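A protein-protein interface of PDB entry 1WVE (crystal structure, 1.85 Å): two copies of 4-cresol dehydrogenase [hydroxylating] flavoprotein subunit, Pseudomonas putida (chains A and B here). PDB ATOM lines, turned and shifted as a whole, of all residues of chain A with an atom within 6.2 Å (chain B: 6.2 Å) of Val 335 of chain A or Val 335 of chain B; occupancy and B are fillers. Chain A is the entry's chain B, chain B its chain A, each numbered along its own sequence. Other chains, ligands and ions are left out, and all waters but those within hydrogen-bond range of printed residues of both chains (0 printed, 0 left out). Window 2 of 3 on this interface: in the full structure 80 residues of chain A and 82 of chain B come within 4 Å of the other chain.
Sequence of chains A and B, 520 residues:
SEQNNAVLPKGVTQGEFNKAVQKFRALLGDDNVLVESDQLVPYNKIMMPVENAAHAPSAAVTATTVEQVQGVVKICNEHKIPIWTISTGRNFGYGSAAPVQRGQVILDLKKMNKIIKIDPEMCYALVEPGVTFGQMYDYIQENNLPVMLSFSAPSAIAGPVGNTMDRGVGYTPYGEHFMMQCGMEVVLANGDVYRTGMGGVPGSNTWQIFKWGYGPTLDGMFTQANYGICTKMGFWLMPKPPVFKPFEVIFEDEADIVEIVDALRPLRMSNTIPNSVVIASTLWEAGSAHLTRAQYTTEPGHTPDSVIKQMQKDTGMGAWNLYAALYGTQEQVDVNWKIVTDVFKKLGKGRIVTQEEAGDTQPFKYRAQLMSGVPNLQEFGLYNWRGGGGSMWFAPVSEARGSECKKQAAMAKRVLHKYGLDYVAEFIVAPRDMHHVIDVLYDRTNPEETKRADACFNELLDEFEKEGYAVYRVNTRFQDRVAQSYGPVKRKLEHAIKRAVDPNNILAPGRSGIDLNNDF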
ATOM      1  N   THR A 272       3.083 -11.139  31.283  1.00  0.00           N
ATOM      2  CA  THR A 272       2.030 -11.297  30.276  1.00  0.00           C
ATOM      3  C   THR A 272       1.220 -10.000  30.235  1.00  0.00           C
ATOM      4  O   THR A 272       0.748  -9.582  29.170  1.00  0.00           O
ATOM      5  CB  THR A 272       1.163 -12.510  30.588  1.00  0.00           C
ATOM      6  OG1 THR A 272       1.976 -13.683  30.434  1.00  0.00           O
ATOM      7  CG2 THR A 272      -0.046 -12.588  29.625  1.00  0.00           C
ATOM      8  N   THR A 329       3.007  -6.695  18.929  1.00  0.00           N
ATOM      9  CA  THR A 329       2.455  -6.886  17.584  1.00  0.00           C
ATOM     10  C   THR A 329       1.046  -7.430  17.785  1.00  0.00           C
ATOM     11  O   THR A 329       0.679  -7.838  18.895  1.00  0.00           O
ATOM     12  CB  THR A 329       3.263  -7.937  16.759  1.00  0.00           C
ATOM     13  OG1 THR A 329       3.155  -9.226  17.383  1.00  0.00           O
ATOM     14  CG2 THR A 329       4.737  -7.540  16.661  1.00  0.00           C
ATOM     15  N   GLN A 330       0.246  -7.451  16.723  1.00  0.00           N
ATOM     16  CA  GLN A 330      -1.105  -7.968  16.858  1.00  0.00           C
ATOM     17  C   GLN A 330      -1.081  -9.413  17.352  1.00  0.00           C
ATOM     18  O   GLN A 330      -1.925  -9.819  18.150  1.00  0.00           O
ATOM     19  CB  GLN A 330      -1.851  -7.916  15.522  1.00  0.00           C
ATOM     20  CG  GLN A 330      -3.330  -8.281  15.671  1.00  0.00           C
ATOM     21  CD  GLN A 330      -4.058  -7.331  16.607  1.00  0.00           C
ATOM     22  OE1 GLN A 330      -3.999  -6.112  16.435  1.00  0.00           O
ATOM     23  NE2 GLN A 330      -4.755  -7.882  17.598  1.00  0.00           N
ATOM     24  N   GLU A 331      -0.110 -10.189  16.875  1.00  0.00           N
ATOM     25  CA  GLU A 331       0.002 -11.595  17.265  1.00  0.00           C
ATOM     26  C   GLU A 331       0.342 -11.784  18.738  1.00  0.00           C
ATOM     27  O   GLU A 331      -0.202 -12.672  19.400  1.00  0.00           O
ATOM     28  CB  GLU A 331       1.053 -12.314  16.404  1.00  0.00           C
ATOM     29  CG  GLU A 331       0.620 -12.528  14.961  1.00  0.00           C
ATOM     30  CD  GLU A 331       0.577 -11.234  14.169  1.00  0.00           C
ATOM     31  OE1 GLU A 331      -0.219 -11.148  13.208  1.00  0.00           O
ATOM     32  OE2 GLU A 331       1.348 -10.306  14.496  1.00  0.00           O
ATOM     33  N   GLN A 332       1.257 -10.963  19.246  1.00  0.00           N
ATOM     34  CA  GLN A 332       1.646 -11.058  20.656  1.00  0.00           C
ATOM     35  C   GLN A 332       0.465 -10.665  21.535  1.00  0.00           C
ATOM     36  O   GLN A 332       0.175 -11.324  22.527  1.00  0.00           O
ATOM     37  CB  GLN A 332       2.840 -10.139  20.946  1.00  0.00           C
ATOM     38  CG  GLN A 332       4.125 -10.519  20.221  1.00  0.00           C
ATOM     39  CD  GLN A 332       5.227  -9.506  20.448  1.00  0.00           C
ATOM     40  OE1 GLN A 332       4.986  -8.294  20.416  1.00  0.00           O
ATOM     41  NE2 GLN A 332       6.449  -9.991  20.670  1.00  0.00           N
ATOM     42  N   VAL A 333      -0.220  -9.589  21.156  1.00  0.00           N
ATOM     43  CA  VAL A 333      -1.378  -9.110  21.902  1.00  0.00           C
ATOM     44  C   VAL A 333      -2.484 -10.167  21.937  1.00  0.00           C
ATOM     45  O   VAL A 333      -3.071 -10.422  22.982  1.00  0.00           O
ATOM     46  CB  VAL A 333      -1.893  -7.798  21.277  1.00  0.00           C
ATOM     47  CG1 VAL A 333      -3.251  -7.409  21.855  1.00  0.00           C
ATOM     48  CG2 VAL A 333      -0.864  -6.690  21.541  1.00  0.00           C
ATOM     49  N   ASP A 334      -2.754 -10.805  20.801  1.00  0.00           N
ATOM     50  CA  ASP A 334      -3.799 -11.832  20.751  1.00  0.00           C
ATOM     51  C   ASP A 334      -3.465 -13.016  21.658  1.00  0.00           C
ATOM     52  O   ASP A 334      -4.315 -13.497  22.402  1.00  0.00           O
ATOM     53  CB  ASP A 334      -3.995 -12.320  19.314  1.00  0.00           C
ATOM     54  CG  ASP A 334      -4.598 -11.256  18.417  1.00  0.00           C
ATOM     55  OD1 ASP A 334      -4.541 -11.414  17.183  1.00  0.00           O
ATOM     56  OD2 ASP A 334      -5.128 -10.260  18.944  1.00  0.00           O
ATOM     57  N   VAL A 335      -2.223 -13.492  21.592  1.00  0.00           N
ATOM     58  CA  VAL A 335      -1.824 -14.613  22.425  1.00  0.00           C
ATOM     59  C   VAL A 335      -1.969 -14.257  23.900  1.00  0.00           C
ATOM     60  O   VAL A 335      -2.468 -15.057  24.689  1.00  0.00           O
ATOM     61  CB  VAL A 335      -0.356 -15.051  22.118  1.00  0.00           C
ATOM     62  CG1 VAL A 335       0.230 -15.846  23.269  1.00  0.00           C
ATOM     63  CG2 VAL A 335      -0.352 -15.933  20.898  1.00  0.00           C
ATOM     64  N   ASN A 336      -1.551 -13.051  24.272  1.00  0.00           N
ATOM     65  CA  ASN A 336      -1.646 -12.642  25.666  1.00  0.00           C
ATOM     66  C   ASN A 336      -3.078 -12.356  26.115  1.00  0.00           C
ATOM     67  O   ASN A 336      -3.419 -12.606  27.270  1.00  0.00           O
ATOM     68  CB  ASN A 336      -0.725 -11.441  25.926  1.00  0.00           C
ATOM     69  CG  ASN A 336       0.746 -11.838  25.913  1.00  0.00           C
ATOM     70  OD1 ASN A 336       1.068 -13.018  26.050  1.00  0.00           O
ATOM     71  ND2 ASN A 336       1.640 -10.861  25.756  1.00  0.00           N
ATOM     72  N   TRP A 337      -3.915 -11.856  25.212  1.00  0.00           N
ATOM     73  CA  TRP A 337      -5.315 -11.581  25.554  1.00  0.00           C
ATOM     74  C   TRP A 337      -6.036 -12.887  25.912  1.00  0.00           C
ATOM     75  O   TRP A 337      -6.883 -12.933  26.813  1.00  0.00           O
ATOM     76  CB  TRP A 337      -6.021 -10.918  24.373  1.00  0.00           C
ATOM     77  CG  TRP A 337      -7.458 -10.556  24.640  1.00  0.00           C
ATOM     78  CD1 TRP A 337      -8.546 -10.917  23.894  1.00  0.00           C
ATOM     79  CD2 TRP A 337      -7.953  -9.702  25.681  1.00  0.00           C
ATOM     80  NE1 TRP A 337      -9.684 -10.337  24.402  1.00  0.00           N
ATOM     81  CE2 TRP A 337      -9.348  -9.583  25.498  1.00  0.00           C
ATOM     82  CE3 TRP A 337      -7.351  -9.023  26.751  1.00  0.00           C
ATOM     83  CZ2 TRP A 337     -10.152  -8.810  26.341  1.00  0.00           C
ATOM     84  CZ3 TRP A 337      -8.153  -8.254  27.593  1.00  0.00           C
ATOM     85  CH2 TRP A 337      -9.540  -8.154  27.380  1.00  0.00           C
ATOM     86  N   LYS A 338      -5.702 -13.951  25.192  1.00  0.00           N
ATOM     87  CA  LYS A 338      -6.308 -15.251  25.441  1.00  0.00           C
ATOM     88  C   LYS A 338      -5.931 -15.720  26.841  1.00  0.00           C
ATOM     89  O   LYS A 338      -6.770 -16.223  27.595  1.00  0.00           O
ATOM     90  CB  LYS A 338      -5.827 -16.257  24.395  1.00  0.00           C
ATOM     91  CG  LYS A 338      -6.333 -17.680  24.594  1.00  0.00           C
ATOM     92  CD  LYS A 338      -7.855 -17.752  24.599  1.00  0.00           C
ATOM     93  CE  LYS A 338      -8.340 -19.181  24.359  1.00  0.00           C
ATOM     94  NZ  LYS A 338      -7.695 -20.165  25.275  1.00  0.00           N
ATOM     95  N   ILE A 339      -4.662 -15.545  27.195  1.00  0.00           N
ATOM     96  CA  ILE A 339      -4.180 -15.940  28.515  1.00  0.00           C
ATOM     97  C   ILE A 339      -4.895 -15.146  29.616  1.00  0.00           C
ATOM     98  O   ILE A 339      -5.331 -15.713  30.628  1.00  0.00           O
ATOM     99  CB  ILE A 339      -2.635 -15.734  28.619  1.00  0.00           C
ATOM    100  CG1 ILE A 339      -1.919 -16.745  27.712  1.00  0.00           C
ATOM    101  CG2 ILE A 339      -2.171 -15.889  30.062  1.00  0.00           C
ATOM    102  CD1 ILE A 339      -0.426 -16.522  27.576  1.00  0.00           C
ATOM    103  N   VAL A 340      -5.019 -13.839  29.415  1.00  0.00           N
ATOM    104  CA  VAL A 340      -5.681 -12.977  30.394  1.00  0.00           C
ATOM    105  C   VAL A 340      -7.159 -13.311  30.531  1.00  0.00           C
ATOM    106  O   VAL A 340      -7.650 -13.523  31.637  1.00  0.00           O
ATOM    107  CB  VAL A 340      -5.550 -11.486  30.014  1.00  0.00           C
ATOM    108  CG1 VAL A 340      -6.422 -10.623  30.929  1.00  0.00           C
ATOM    109  CG2 VAL A 340      -4.098 -11.068  30.113  1.00  0.00           C
ATOM    110  N   THR B 272      10.893  -8.936  22.952  1.00  0.00           N
ATOM    111  CA  THR B 272      10.523 -10.137  22.200  1.00  0.00           C
ATOM    112  C   THR B 272      11.569 -11.208  22.524  1.00  0.00           C
ATOM    113  O   THR B 272      11.253 -12.397  22.624  1.00  0.00           O
ATOM    114  CB  THR B 272      10.457  -9.846  20.689  1.00  0.00           C
ATOM    115  OG1 THR B 272       9.383  -8.923  20.447  1.00  0.00           O
ATOM    116  CG2 THR B 272      10.203 -11.142  19.896  1.00  0.00           C
ATOM    117  N   THR B 329       4.598 -19.416  27.656  1.00  0.00           N
ATOM    118  CA  THR B 329       3.759 -20.555  27.294  1.00  0.00           C
ATOM    119  C   THR B 329       4.152 -20.938  25.874  1.00  0.00           C
ATOM    120  O   THR B 329       4.862 -20.183  25.197  1.00  0.00           O
ATOM    121  CB  THR B 329       2.261 -20.202  27.309  1.00  0.00           C
ATOM    122  OG1 THR B 329       1.987 -19.263  26.270  1.00  0.00           O
ATOM    123  CG2 THR B 329       1.871 -19.599  28.660  1.00  0.00           C
ATOM    124  N   GLN B 330       3.708 -22.106  25.414  1.00  0.00           N
ATOM    125  CA  GLN B 330       4.059 -22.532  24.063  1.00  0.00           C
ATOM    126  C   GLN B 330       3.602 -21.505  23.044  1.00  0.00           C
ATOM    127  O   GLN B 330       4.326 -21.203  22.095  1.00  0.00           O
ATOM    128  CB  GLN B 330       3.427 -23.881  23.722  1.00  0.00           C
ATOM    129  CG  GLN B 330       3.922 -24.425  22.387  1.00  0.00           C
ATOM    130  CD  GLN B 330       5.404 -24.738  22.423  1.00  0.00           C
ATOM    131  OE1 GLN B 330       5.849 -25.554  23.226  1.00  0.00           O
ATOM    132  NE2 GLN B 330       6.178 -24.086  21.559  1.00  0.00           N
ATOM    133  N   GLU B 331       2.404 -20.966  23.246  1.00  0.00           N
ATOM    134  CA  GLU B 331       1.854 -19.970  22.329  1.00  0.00           C
ATOM    135  C   GLU B 331       2.675 -18.691  22.288  1.00  0.00           C
ATOM    136  O   GLU B 331       2.912 -18.124  21.216  1.00  0.00           O
ATOM    137  CB  GLU B 331       0.408 -19.632  22.702  1.00  0.00           C
ATOM    138  CG  GLU B 331      -0.566 -20.772  22.467  1.00  0.00           C
ATOM    139  CD  GLU B 331      -0.433 -21.893  23.484  1.00  0.00           C
ATOM    140  OE1 GLU B 331      -0.949 -22.991  23.204  1.00  0.00           O
ATOM    141  OE2 GLU B 331       0.172 -21.682  24.564  1.00  0.00           O
ATOM    142  N   GLN B 332       3.106 -18.218  23.454  1.00  0.00           N
ATOM    143  CA  GLN B 332       3.909 -16.998  23.481  1.00  0.00           C
ATOM    144  C   GLN B 332       5.224 -17.245  22.767  1.00  0.00           C
ATOM    145  O   GLN B 332       5.662 -16.421  21.974  1.00  0.00           O
ATOM    146  CB  GLN B 332       4.176 -16.548  24.922  1.00  0.00           C
ATOM    147  CG  GLN B 332       2.943 -16.041  25.642  1.00  0.00           C
ATOM    148  CD  GLN B 332       3.209 -15.762  27.105  1.00  0.00           C
ATOM    149  OE1 GLN B 332       3.893 -16.535  27.776  1.00  0.00           O
ATOM    150  NE2 GLN B 332       2.658 -14.662  27.611  1.00  0.00           N
ATOM    151  N   VAL B 333       5.841 -18.390  23.044  1.00  0.00           N
ATOM    152  CA  VAL B 333       7.114 -18.749  22.421  1.00  0.00           C
ATOM    153  C   VAL B 333       7.003 -18.854  20.897  1.00  0.00           C
ATOM    154  O   VAL B 333       7.878 -18.373  20.170  1.00  0.00           O
ATOM    155  CB  VAL B 333       7.648 -20.083  22.998  1.00  0.00           C
ATOM    156  CG1 VAL B 333       8.827 -20.586  22.170  1.00  0.00           C
ATOM    157  CG2 VAL B 333       8.066 -19.882  24.452  1.00  0.00           C
ATOM    158  N   ASP B 334       5.933 -19.478  20.415  1.00  0.00           N
ATOM    159  CA  ASP B 334       5.719 -19.618  18.976  1.00  0.00           C
ATOM    160  C   ASP B 334       5.556 -18.261  18.299  1.00  0.00           C
ATOM    161  O   ASP B 334       6.170 -17.999  17.266  1.00  0.00           O
ATOM    162  CB  ASP B 334       4.484 -20.483  18.710  1.00  0.00           C
ATOM    163  CG  ASP B 334       4.682 -21.935  19.137  1.00  0.00           C
ATOM    164  OD1 ASP B 334       3.672 -22.662  19.221  1.00  0.00           O
ATOM    165  OD2 ASP B 334       5.840 -22.348  19.384  1.00  0.00           O
ATOM    166  N   VAL B 335       4.729 -17.391  18.873  1.00  0.00           N
ATOM    167  CA  VAL B 335       4.537 -16.074  18.286  1.00  0.00           C
ATOM    168  C   VAL B 335       5.861 -15.332  18.208  1.00  0.00           C
ATOM    169  O   VAL B 335       6.189 -14.750  17.173  1.00  0.00           O
ATOM    170  CB  VAL B 335       3.532 -15.215  19.093  1.00  0.00           C
ATOM    171  CG1 VAL B 335       3.616 -13.756  18.647  1.00  0.00           C
ATOM    172  CG2 VAL B 335       2.123 -15.726  18.865  1.00  0.00           C
ATOM    173  N   ASN B 336       6.638 -15.354  19.293  1.00  0.00           N
ATOM    174  CA  ASN B 336       7.921 -14.657  19.284  1.00  0.00           C
ATOM    175  C   ASN B 336       8.966 -15.326  18.392  1.00  0.00           C
ATOM    176  O   ASN B 336       9.814 -14.645  17.827  1.00  0.00           O
ATOM    177  CB  ASN B 336       8.470 -14.497  20.705  1.00  0.00           C
ATOM    178  CG  ASN B 336       7.653 -13.523  21.536  1.00  0.00           C
ATOM    179  OD1 ASN B 336       6.990 -12.637  21.001  1.00  0.00           O
ATOM    180  ND2 ASN B 336       7.713 -13.678  22.853  1.00  0.00           N
ATOM    181  N   TRP B 337       8.909 -16.648  18.257  1.00  0.00           N
ATOM    182  CA  TRP B 337       9.863 -17.350  17.396  1.00  0.00           C
ATOM    183  C   TRP B 337       9.669 -16.905  15.939  1.00  0.00           C
ATOM    184  O   TRP B 337      10.637 -16.726  15.196  1.00  0.00           O
ATOM    185  CB  TRP B 337       9.669 -18.869  17.514  1.00  0.00           C
ATOM    186  CG  TRP B 337      10.650 -19.698  16.700  1.00  0.00           C
ATOM    187  CD1 TRP B 337      10.339 -20.674  15.793  1.00  0.00           C
ATOM    188  CD2 TRP B 337      12.084 -19.661  16.767  1.00  0.00           C
ATOM    189  NE1 TRP B 337      11.487 -21.248  15.297  1.00  0.00           N
ATOM    190  CE2 TRP B 337      12.572 -20.644  15.878  1.00  0.00           C
ATOM    191  CE3 TRP B 337      13.005 -18.894  17.494  1.00  0.00           C
ATOM    192  CZ2 TRP B 337      13.938 -20.882  15.697  1.00  0.00           C
ATOM    193  CZ3 TRP B 337      14.365 -19.129  17.315  1.00  0.00           C
ATOM    194  CH2 TRP B 337      14.818 -20.116  16.423  1.00  0.00           C
ATOM    195  N   LYS B 338       8.412 -16.715  15.544  1.00  0.00           N
ATOM    196  CA  LYS B 338       8.092 -16.276  14.186  1.00  0.00           C
ATOM    197  C   LYS B 338       8.696 -14.892  13.958  1.00  0.00           C
ATOM    198  O   LYS B 338       9.298 -14.633  12.921  1.00  0.00           O
ATOM    199  CB  LYS B 338       6.568 -16.235  13.993  1.00  0.00           C
ATOM    200  CG  LYS B 338       6.086 -15.736  12.615  1.00  0.00           C
ATOM    201  CD  LYS B 338       6.627 -16.606  11.483  1.00  0.00           C
ATOM    202  CE  LYS B 338       5.861 -16.404  10.176  1.00  0.00           C
ATOM    203  NZ  LYS B 338       5.992 -15.041   9.603  1.00  0.00           N
ATOM    204  N   ILE B 339       8.546 -14.005  14.940  1.00  0.00           N
ATOM    205  CA  ILE B 339       9.083 -12.657  14.833  1.00  0.00           C
ATOM    206  C   ILE B 339      10.608 -12.679  14.700  1.00  0.00           C
ATOM    207  O   ILE B 339      11.179 -11.965  13.867  1.00  0.00           O
ATOM    208  CB  ILE B 339       8.698 -11.814  16.066  1.00  0.00           C
ATOM    209  CG1 ILE B 339       7.191 -11.521  16.037  1.00  0.00           C
ATOM    210  CG2 ILE B 339       9.514 -10.528  16.092  1.00  0.00           C
ATOM    211  CD1 ILE B 339       6.654 -10.907  17.310  1.00  0.00           C
ATOM    212  N   VAL B 340      11.262 -13.499  15.523  1.00  0.00           N
ATOM    213  CA  VAL B 340      12.719 -13.598  15.506  1.00  0.00           C
ATOM    214  C   VAL B 340      13.225 -14.184  14.196  1.00  0.00           C
ATOM    215  O   VAL B 340      14.097 -13.609  13.547  1.00  0.00           O
ATOM    216  CB  VAL B 340      13.242 -14.467  16.677  1.00  0.00           C
ATOM    217  CG1 VAL B 340      14.725 -14.750  16.497  1.00  0.00           C
ATOM    218  CG2 VAL B 340      13.007 -13.753  17.999  1.00  0.00           C
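OG1 of Thr 329 of chain A touches CD1 of Ile 339 of chain B, 3.9 Å away.
CB of Glu 331 of chain A touches CG1 of Val 335 of chain B (3.7 Å).
CG1 of Val 335 of chain B touches CG of Gln 332 of chain A (3.6 Å).
CD1 of Ile 339 of chain B touches NE2 of Gln 332 of chain A, at 3.5 Å.
CG1 of Val 335 of chain A touches CB of Glu 331 of chain B (3.8 Å).
CG of Gln 332 of chain B touches CG1 of Val 335 of chain A (3.6 Å).
Val 335 of chain A touches Val 335 of chain B (CG2 to CG2, 3.2 Å).
CD1 of Ile 339 of chain A touches OG1 of Thr 329 of chain B, at 3.9 Å.
Ile 339 of chain A touches Gln 332 of chain B.
OG1 of Thr 272 of chain B is in hydrogen-bond range of NE2 of Gln 332 of chain A (3.1 Å).
The side-chain hydroxyl (OG1) of Thr 272 of chain A sits at hydrogen-bond distance from the side-chain amide nitrogen (NE2) of Gln 332 of chain B (3.1 Å).
NE2 of Gln 332 of chain B lies within hydrogen-bond range of OD1 of Asn 336 of chain A (2.8 Å).
The side-chain amide oxygen of Asn 336 of chain B sits at hydrogen-bond distance from the side-chain amide nitrogen of Gln 332 of chain A.
Of the 13 printed residues of chain B, 7 touch a printed residue of chain A.
Hydrophobic or aromatic side chains of chain B that line the printed part of chain A: Val 335 and Ile 339.
Of the 13 printed residues of chain A, 7 touch a printed residue of chain B.
Printed residues of chain A that touch a printed residue of chain B: Thr 272, Thr 329, Glu 331, Gln 332, Val 335, Asn 336 and Ile 339.
Hydrophobic or aromatic side chains of chain A that line the printed part of chain B: Val 335 and Ile 339.
Among the printed residues, 13 pairs touch across the chains.
Among the printed residues, no Asp or Glu carboxylate lies within 4 Å of a Lys or Arg side-chain nitrogen of the other chain.
Thr 329 of chain A touches Ile 339 of chain B, and with the chains exchanged Ile 339 of chain A touches Thr 329 of chain B.
Glu 331 of chain A touches Val 335 of chain B, and with the chains exchanged Val 335 of chain A touches Glu 331 of chain B.
Gln 332 of chain A touches Asn 336 of chain B, and with the chains exchanged Asn 336 of chain A touches Gln 332 of chain B.
Val 335 of chain B touches its own counterpart, Val 335 of chain A.
Positions printed for both chains: 272, 329, 330, 331, 332, 333, 334, 335, 336, 337, 338, 339 and 340.
Of the printed residues of chain B, Thr 272 of chain A touches Gln 332 (3.1 Å).
Of chain B, only Glu 331 (3.8 Å), Gln 332 (3.6 Å) and Val 335 (3.2 Å) come within 4 Å of Val 335 of chain A.
Val 340 of chain A touches none of the printed residues of chain B.
Printed residues of chain A within 4 Å of Thr 329 of chain B: Ile 339 (3.9 Å).
Val 335 of chain B touches just these residues of chain A: Glu 331, Gln 332 and Val 335.
The nearest residue of chain B that does not touch Val 335 of chain A is Thr 329 of chain B (4.9 Å).
The nearest residue of chain A that does not touch Val 335 of chain B is Thr 329 of chain A (4.7 Å).
The side-chain carboxylate of Glu 331 of chain B sits at hydrogen-bond distance from the side-chain hydroxyl of Thr 329 of chain B (3.5 Å).
N of Thr 329 of chain B sits at hydrogen-bond distance from OE1 of Gln 332 of chain B, 3.0 Å away.
OG1 of Thr 329 of chain A sits close to N of Glu 331 of chain A.
OE1 of Gln 332 of chain A is in hydrogen-bond range of N of Thr 329 of chain A (2.9 Å).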
